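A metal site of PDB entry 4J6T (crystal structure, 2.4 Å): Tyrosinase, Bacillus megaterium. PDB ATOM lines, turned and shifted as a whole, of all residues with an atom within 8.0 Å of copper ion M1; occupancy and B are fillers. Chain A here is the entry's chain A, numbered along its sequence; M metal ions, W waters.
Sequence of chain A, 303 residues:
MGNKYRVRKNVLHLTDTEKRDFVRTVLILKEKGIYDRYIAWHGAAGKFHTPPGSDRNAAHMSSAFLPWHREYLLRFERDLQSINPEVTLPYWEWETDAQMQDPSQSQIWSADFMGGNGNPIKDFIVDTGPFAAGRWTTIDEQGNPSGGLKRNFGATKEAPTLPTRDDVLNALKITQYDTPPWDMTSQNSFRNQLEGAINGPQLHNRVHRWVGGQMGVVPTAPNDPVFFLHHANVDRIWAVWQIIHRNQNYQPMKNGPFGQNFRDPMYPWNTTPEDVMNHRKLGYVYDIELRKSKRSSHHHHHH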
ATOM      1  N   HIS A  42      25.307  17.737  -0.515  1.00  0.00           N
ATOM      2  CA  HIS A  42      24.834  17.047   0.665  1.00  0.00           C
ATOM      3  C   HIS A  42      23.344  16.711   0.577  1.00  0.00           C
ATOM      4  O   HIS A  42      22.934  15.582   0.836  1.00  0.00           O
ATOM      5  CB  HIS A  42      25.133  17.845   1.919  1.00  0.00           C
ATOM      6  CG  HIS A  42      24.852  17.115   3.181  1.00  0.00           C
ATOM      7  ND1 HIS A  42      23.803  17.429   4.016  1.00  0.00           N
ATOM      8  CD2 HIS A  42      25.468  16.040   3.741  1.00  0.00           C
ATOM      9  CE1 HIS A  42      23.797  16.607   5.050  1.00  0.00           C
ATOM     10  NE2 HIS A  42      24.804  15.757   4.907  1.00  0.00           N
ATOM     11  N   GLY A  43      22.534  17.695   0.202  1.00  0.00           N
ATOM     12  CA  GLY A  43      21.123  17.437  -0.033  1.00  0.00           C
ATOM     13  C   GLY A  43      20.927  16.376  -1.107  1.00  0.00           C
ATOM     14  O   GLY A  43      20.076  15.488  -0.962  1.00  0.00           O
ATOM     15  N   ALA A  45      22.766  13.860  -2.001  1.00  0.00           N
ATOM     16  CA  ALA A  45      23.044  12.498  -1.559  1.00  0.00           C
ATOM     17  C   ALA A  45      21.884  11.895  -0.743  1.00  0.00           C
ATOM     18  O   ALA A  45      21.632  10.674  -0.801  1.00  0.00           O
ATOM     19  CB  ALA A  45      24.333  12.479  -0.757  1.00  0.00           C
ATOM     20  N   ASN A  57      20.579   5.980   2.441  1.00  0.00           N
ATOM     21  CA  ASN A  57      20.985   6.810   1.304  1.00  0.00           C
ATOM     22  C   ASN A  57      22.516   6.934   1.176  1.00  0.00           C
ATOM     23  O   ASN A  57      23.263   6.404   2.006  1.00  0.00           O
ATOM     24  CB  ASN A  57      20.273   8.179   1.287  1.00  0.00           C
ATOM     25  CG  ASN A  57      20.638   9.036   2.472  1.00  0.00           C
ATOM     26  OD1 ASN A  57      21.727   9.609   2.514  1.00  0.00           O
ATOM     27  ND2 ASN A  57      19.726   9.136   3.433  1.00  0.00           N
ATOM     28  N   ALA A  59      24.762   9.104   1.724  1.00  0.00           N
ATOM     29  CA  ALA A  59      25.585   9.749   2.745  1.00  0.00           C
ATOM     30  C   ALA A  59      25.149   9.420   4.176  1.00  0.00           C
ATOM     31  O   ALA A  59      25.915   9.655   5.112  1.00  0.00           O
ATOM     32  CB  ALA A  59      25.584  11.246   2.525  1.00  0.00           C
ATOM     33  N   HIS A  60      23.938   8.911   4.357  1.00  0.00           N
ATOM     34  CA  HIS A  60      23.429   8.676   5.695  1.00  0.00           C
ATOM     35  C   HIS A  60      22.643   7.405   5.812  1.00  0.00           C
ATOM     36  O   HIS A  60      21.993   6.944   4.845  1.00  0.00           O
ATOM     37  CB  HIS A  60      22.583   9.854   6.151  1.00  0.00           C
ATOM     38  CG  HIS A  60      23.192  11.203   5.862  1.00  0.00           C
ATOM     39  ND1 HIS A  60      23.067  11.809   4.666  1.00  0.00           N
ATOM     40  CD2 HIS A  60      23.969  12.052   6.653  1.00  0.00           C
ATOM     41  CE1 HIS A  60      23.716  12.986   4.692  1.00  0.00           C
ATOM     42  NE2 HIS A  60      24.265  13.139   5.910  1.00  0.00           N
ATOM     43  N   PHE A  65      28.312   6.409   5.388  1.00  0.00           N
ATOM     44  CA  PHE A  65      28.227   7.645   6.180  1.00  0.00           C
ATOM     45  C   PHE A  65      29.591   8.236   6.484  1.00  0.00           C
ATOM     46  O   PHE A  65      29.834   9.417   6.199  1.00  0.00           O
ATOM     47  CB  PHE A  65      27.494   7.401   7.488  1.00  0.00           C
ATOM     48  CG  PHE A  65      27.621   8.542   8.488  1.00  0.00           C
ATOM     49  CD1 PHE A  65      27.007   9.762   8.245  1.00  0.00           C
ATOM     50  CD2 PHE A  65      28.340   8.369   9.662  1.00  0.00           C
ATOM     51  CE1 PHE A  65      27.095  10.808   9.163  1.00  0.00           C
ATOM     52  CE2 PHE A  65      28.437   9.406  10.592  1.00  0.00           C
ATOM     53  CZ  PHE A  65      27.815  10.635  10.337  1.00  0.00           C
ATOM     54  N   TRP A  68      31.915   8.964   3.034  1.00  0.00           N
ATOM     55  CA  TRP A  68      31.282  10.056   2.285  1.00  0.00           C
ATOM     56  C   TRP A  68      31.640  11.408   2.905  1.00  0.00           C
ATOM     57  O   TRP A  68      32.187  12.312   2.240  1.00  0.00           O
ATOM     58  CB  TRP A  68      29.760   9.874   2.216  1.00  0.00           C
ATOM     59  CG  TRP A  68      29.018  10.760   1.238  1.00  0.00           C
ATOM     60  CD1 TRP A  68      28.499  10.384   0.026  1.00  0.00           C
ATOM     61  CD2 TRP A  68      28.692  12.154   1.395  1.00  0.00           C
ATOM     62  NE1 TRP A  68      27.860  11.443  -0.562  1.00  0.00           N
ATOM     63  CE2 TRP A  68      27.966  12.536   0.246  1.00  0.00           C
ATOM     64  CE3 TRP A  68      28.918  13.103   2.399  1.00  0.00           C
ATOM     65  CZ2 TRP A  68      27.491  13.847   0.053  1.00  0.00           C
ATOM     66  CZ3 TRP A  68      28.439  14.407   2.212  1.00  0.00           C
ATOM     67  CH2 TRP A  68      27.736  14.759   1.049  1.00  0.00           C
ATOM     68  N   HIS A  69      31.343  11.560   4.194  1.00  0.00           N
ATOM     69  CA  HIS A  69      31.676  12.797   4.872  1.00  0.00           C
ATOM     70  C   HIS A  69      33.176  13.090   4.880  1.00  0.00           C
ATOM     71  O   HIS A  69      33.583  14.242   4.748  1.00  0.00           O
ATOM     72  CB  HIS A  69      31.014  12.880   6.244  1.00  0.00           C
ATOM     73  CG  HIS A  69      29.526  13.077   6.171  1.00  0.00           C
ATOM     74  ND1 HIS A  69      28.652  12.036   5.951  1.00  0.00           N
ATOM     75  CD2 HIS A  69      28.768  14.193   6.250  1.00  0.00           C
ATOM     76  CE1 HIS A  69      27.412  12.502   5.923  1.00  0.00           C
ATOM     77  NE2 HIS A  69      27.455  13.808   6.108  1.00  0.00           N
ATOM     78  N   TYR A  72      33.865  14.520   1.614  1.00  0.00           N
ATOM     79  CA  TYR A  72      33.227  15.819   1.593  1.00  0.00           C
ATOM     80  C   TYR A  72      34.128  16.871   2.229  1.00  0.00           C
ATOM     81  O   TYR A  72      34.311  17.966   1.679  1.00  0.00           O
ATOM     82  CB  TYR A  72      31.937  15.721   2.390  1.00  0.00           C
ATOM     83  CG  TYR A  72      30.984  16.902   2.333  1.00  0.00           C
ATOM     84  CD1 TYR A  72      30.249  17.187   1.178  1.00  0.00           C
ATOM     85  CD2 TYR A  72      30.755  17.672   3.471  1.00  0.00           C
ATOM     86  CE1 TYR A  72      29.350  18.227   1.145  1.00  0.00           C
ATOM     87  CE2 TYR A  72      29.838  18.719   3.448  1.00  0.00           C
ATOM     88  CZ  TYR A  72      29.134  18.994   2.288  1.00  0.00           C
ATOM     89  OH  TYR A  72      28.227  20.030   2.291  1.00  0.00           O
ATOM     90  N   GLU A 195      27.347   7.326  14.146  1.00  0.00           N
ATOM     91  CA  GLU A 195      26.300   8.073  13.480  1.00  0.00           C
ATOM     92  C   GLU A 195      25.199   8.389  14.493  1.00  0.00           C
ATOM     93  O   GLU A 195      24.618   9.477  14.492  1.00  0.00           O
ATOM     94  CB  GLU A 195      25.752   7.325  12.265  1.00  0.00           C
ATOM     95  CG  GLU A 195      24.900   8.222  11.364  1.00  0.00           C
ATOM     96  CD  GLU A 195      24.390   7.548  10.078  1.00  0.00           C
ATOM     97  OE1 GLU A 195      23.811   8.263   9.223  1.00  0.00           O
ATOM     98  OE2 GLU A 195      24.547   6.315   9.919  1.00  0.00           O
ATOM     99  N   HIS A 204      26.770  11.720  16.727  1.00  0.00           N
ATOM    100  CA  HIS A 204      26.550  12.561  15.554  1.00  0.00           C
ATOM    101  C   HIS A 204      25.135  13.130  15.436  1.00  0.00           C
ATOM    102  O   HIS A 204      24.960  14.345  15.357  1.00  0.00           O
ATOM    103  CB  HIS A 204      26.902  11.811  14.270  1.00  0.00           C
ATOM    104  CG  HIS A 204      26.395  12.468  13.019  1.00  0.00           C
ATOM    105  ND1 HIS A 204      25.280  12.032  12.339  1.00  0.00           N
ATOM    106  CD2 HIS A 204      26.851  13.547  12.338  1.00  0.00           C
ATOM    107  CE1 HIS A 204      25.078  12.800  11.289  1.00  0.00           C
ATOM    108  NE2 HIS A 204      26.029  13.733  11.263  1.00  0.00           N
ATOM    109  N   ASN A 205      24.129  12.252  15.419  1.00  0.00           N
ATOM    110  CA  ASN A 205      22.751  12.715  15.347  1.00  0.00           C
ATOM    111  C   ASN A 205      22.410  13.698  16.463  1.00  0.00           C
ATOM    112  O   ASN A 205      21.658  14.658  16.252  1.00  0.00           O
ATOM    113  CB  ASN A 205      21.762  11.544  15.385  1.00  0.00           C
ATOM    114  CG  ASN A 205      21.783  10.706  14.114  1.00  0.00           C
ATOM    115  OD1 ASN A 205      22.208  11.182  13.050  1.00  0.00           O
ATOM    116  ND2 ASN A 205      21.312   9.451  14.202  1.00  0.00           N
ATOM    117  N   HIS A 208      23.674  17.371  15.870  1.00  0.00           N
ATOM    118  CA  HIS A 208      22.734  18.012  14.961  1.00  0.00           C
ATOM    119  C   HIS A 208      21.469  18.529  15.669  1.00  0.00           C
ATOM    120  O   HIS A 208      21.056  19.674  15.452  1.00  0.00           O
ATOM    121  CB  HIS A 208      22.336  17.027  13.847  1.00  0.00           C
ATOM    122  CG  HIS A 208      23.360  16.915  12.764  1.00  0.00           C
ATOM    123  ND1 HIS A 208      23.489  17.835  11.747  1.00  0.00           N
ATOM    124  CD2 HIS A 208      24.315  15.973  12.534  1.00  0.00           C
ATOM    125  CE1 HIS A 208      24.473  17.472  10.948  1.00  0.00           C
ATOM    126  NE2 HIS A 208      24.986  16.345  11.395  1.00  0.00           N
ATOM    127  N   VAL A 218      18.743  17.642   8.500  1.00  0.00           N
ATOM    128  CA  VAL A 218      19.860  17.144   7.688  1.00  0.00           C
ATOM    129  C   VAL A 218      20.093  17.847   6.327  1.00  0.00           C
ATOM    130  O   VAL A 218      21.215  18.242   6.044  1.00  0.00           O
ATOM    131  CB  VAL A 218      19.816  15.607   7.468  1.00  0.00           C
ATOM    132  CG1 VAL A 218      21.135  15.112   6.845  1.00  0.00           C
ATOM    133  CG2 VAL A 218      19.515  14.902   8.786  1.00  0.00           C
ATOM    134  N   PRO A 219      19.031  18.022   5.511  1.00  0.00           N
ATOM    135  CA  PRO A 219      19.295  18.616   4.187  1.00  0.00           C
ATOM    136  C   PRO A 219      19.687  20.117   4.201  1.00  0.00           C
ATOM    137  O   PRO A 219      20.205  20.627   3.213  1.00  0.00           O
ATOM    138  CB  PRO A 219      17.965  18.428   3.437  1.00  0.00           C
ATOM    139  CG  PRO A 219      17.233  17.343   4.209  1.00  0.00           C
ATOM    140  CD  PRO A 219      17.640  17.532   5.627  1.00  0.00           C
ATOM    141  N   ALA A 221      21.565  21.310   6.837  1.00  0.00           N
ATOM    142  CA  ALA A 221      22.664  21.384   7.816  1.00  0.00           C
ATOM    143  C   ALA A 221      23.971  22.117   7.394  1.00  0.00           C
ATOM    144  O   ALA A 221      24.495  22.924   8.167  1.00  0.00           O
ATOM    145  CB  ALA A 221      22.957  19.990   8.389  1.00  0.00           C
ATOM    146  N   PRO A 222      24.491  21.858   6.174  1.00  0.00           N
ATOM    147  CA  PRO A 222      25.721  22.576   5.778  1.00  0.00           C
ATOM    148  C   PRO A 222      25.628  24.103   5.694  1.00  0.00           C
ATOM    149  O   PRO A 222      26.670  24.757   5.631  1.00  0.00           O
ATOM    150  CB  PRO A 222      26.055  21.965   4.402  1.00  0.00           C
ATOM    151  CG  PRO A 222      25.463  20.551   4.493  1.00  0.00           C
ATOM    152  CD  PRO A 222      24.189  20.731   5.259  1.00  0.00           C
ATOM    153  N   PHE A 227      28.830  22.939  10.739  1.00  0.00           N
ATOM    154  CA  PHE A 227      28.608  21.601  10.171  1.00  0.00           C
ATOM    155  C   PHE A 227      29.935  20.885   9.858  1.00  0.00           C
ATOM    156  O   PHE A 227      30.077  19.692  10.117  1.00  0.00           O
ATOM    157  CB  PHE A 227      27.745  21.691   8.891  1.00  0.00           C
ATOM    158  CG  PHE A 227      27.556  20.369   8.165  1.00  0.00           C
ATOM    159  CD1 PHE A 227      28.455  19.960   7.194  1.00  0.00           C
ATOM    160  CD2 PHE A 227      26.488  19.531   8.491  1.00  0.00           C
ATOM    161  CE1 PHE A 227      28.298  18.740   6.552  1.00  0.00           C
ATOM    162  CE2 PHE A 227      26.318  18.313   7.842  1.00  0.00           C
ATOM    163  CZ  PHE A 227      27.227  17.914   6.872  1.00  0.00           C
ATOM    164  N   HIS A 230      31.943  20.275  13.050  1.00  0.00           N
ATOM    165  CA  HIS A 230      31.385  19.109  13.707  1.00  0.00           C
ATOM    166  C   HIS A 230      31.808  17.810  13.008  1.00  0.00           C
ATOM    167  O   HIS A 230      32.188  16.827  13.670  1.00  0.00           O
ATOM    168  CB  HIS A 230      29.878  19.173  13.724  1.00  0.00           C
ATOM    169  CG  HIS A 230      29.236  17.831  13.909  1.00  0.00           C
ATOM    170  ND1 HIS A 230      28.415  17.258  12.956  1.00  0.00           N
ATOM    171  CD2 HIS A 230      29.356  16.930  14.904  1.00  0.00           C
ATOM    172  CE1 HIS A 230      28.011  16.075  13.393  1.00  0.00           C
ATOM    173  NE2 HIS A 230      28.570  15.850  14.568  1.00  0.00           N
ATOM    174  N   HIS A 231      31.720  17.821  11.675  1.00  0.00           N
ATOM    175  CA  HIS A 231      32.015  16.608  10.917  1.00  0.00           C
ATOM    176  C   HIS A 231      33.496  16.264  10.954  1.00  0.00           C
ATOM    177  O   HIS A 231      33.871  15.099  10.920  1.00  0.00           O
ATOM    178  CB  HIS A 231      31.459  16.678   9.495  1.00  0.00           C
ATOM    179  CG  HIS A 231      30.116  16.047   9.377  1.00  0.00           C
ATOM    180  ND1 HIS A 231      29.944  14.683   9.282  1.00  0.00           N
ATOM    181  CD2 HIS A 231      28.871  16.592   9.418  1.00  0.00           C
ATOM    182  CE1 HIS A 231      28.652  14.409   9.255  1.00  0.00           C
ATOM    183  NE2 HIS A 231      27.982  15.549   9.321  1.00  0.00           N
HETATM  184 CU    CU M   1      25.422  14.643   6.661  1.00  0.00          CU
HETATM  185 CU    CU M   2      25.768  15.242   9.634  1.00  0.00          CU
HETATM  186  O   HOH W   1      23.874  15.744   8.541  1.00  0.00           O
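Merely in contact with copper ion M1: Phe 227 and His 231. Within 4 Å of copper ion M1: His 42, His 60, His 69, Phe 227 and His 231. The nearest printed residue that does not touch copper ion M1 is Val 218 (4.3 Å).
ND1 of His 42 lies close to O of Val 218 (3.4 Å). ND1 of His 69 sits at hydrogen-bond distance from O of Phe 65, 2.9 Å away. N of His 60 is in hydrogen-bond range of OD1 of Asn 57, at 3.0 Å.
Copper ion M1 is bound by a ring nitrogen (NE2) of His 60, a ring nitrogen (NE2) of His 42 and a ring nitrogen (NE2) of His 69. Copper ion M1 has three donor atoms within binding distance. Slightly farther from copper ion M1 lies water W1 (2.7 Å).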
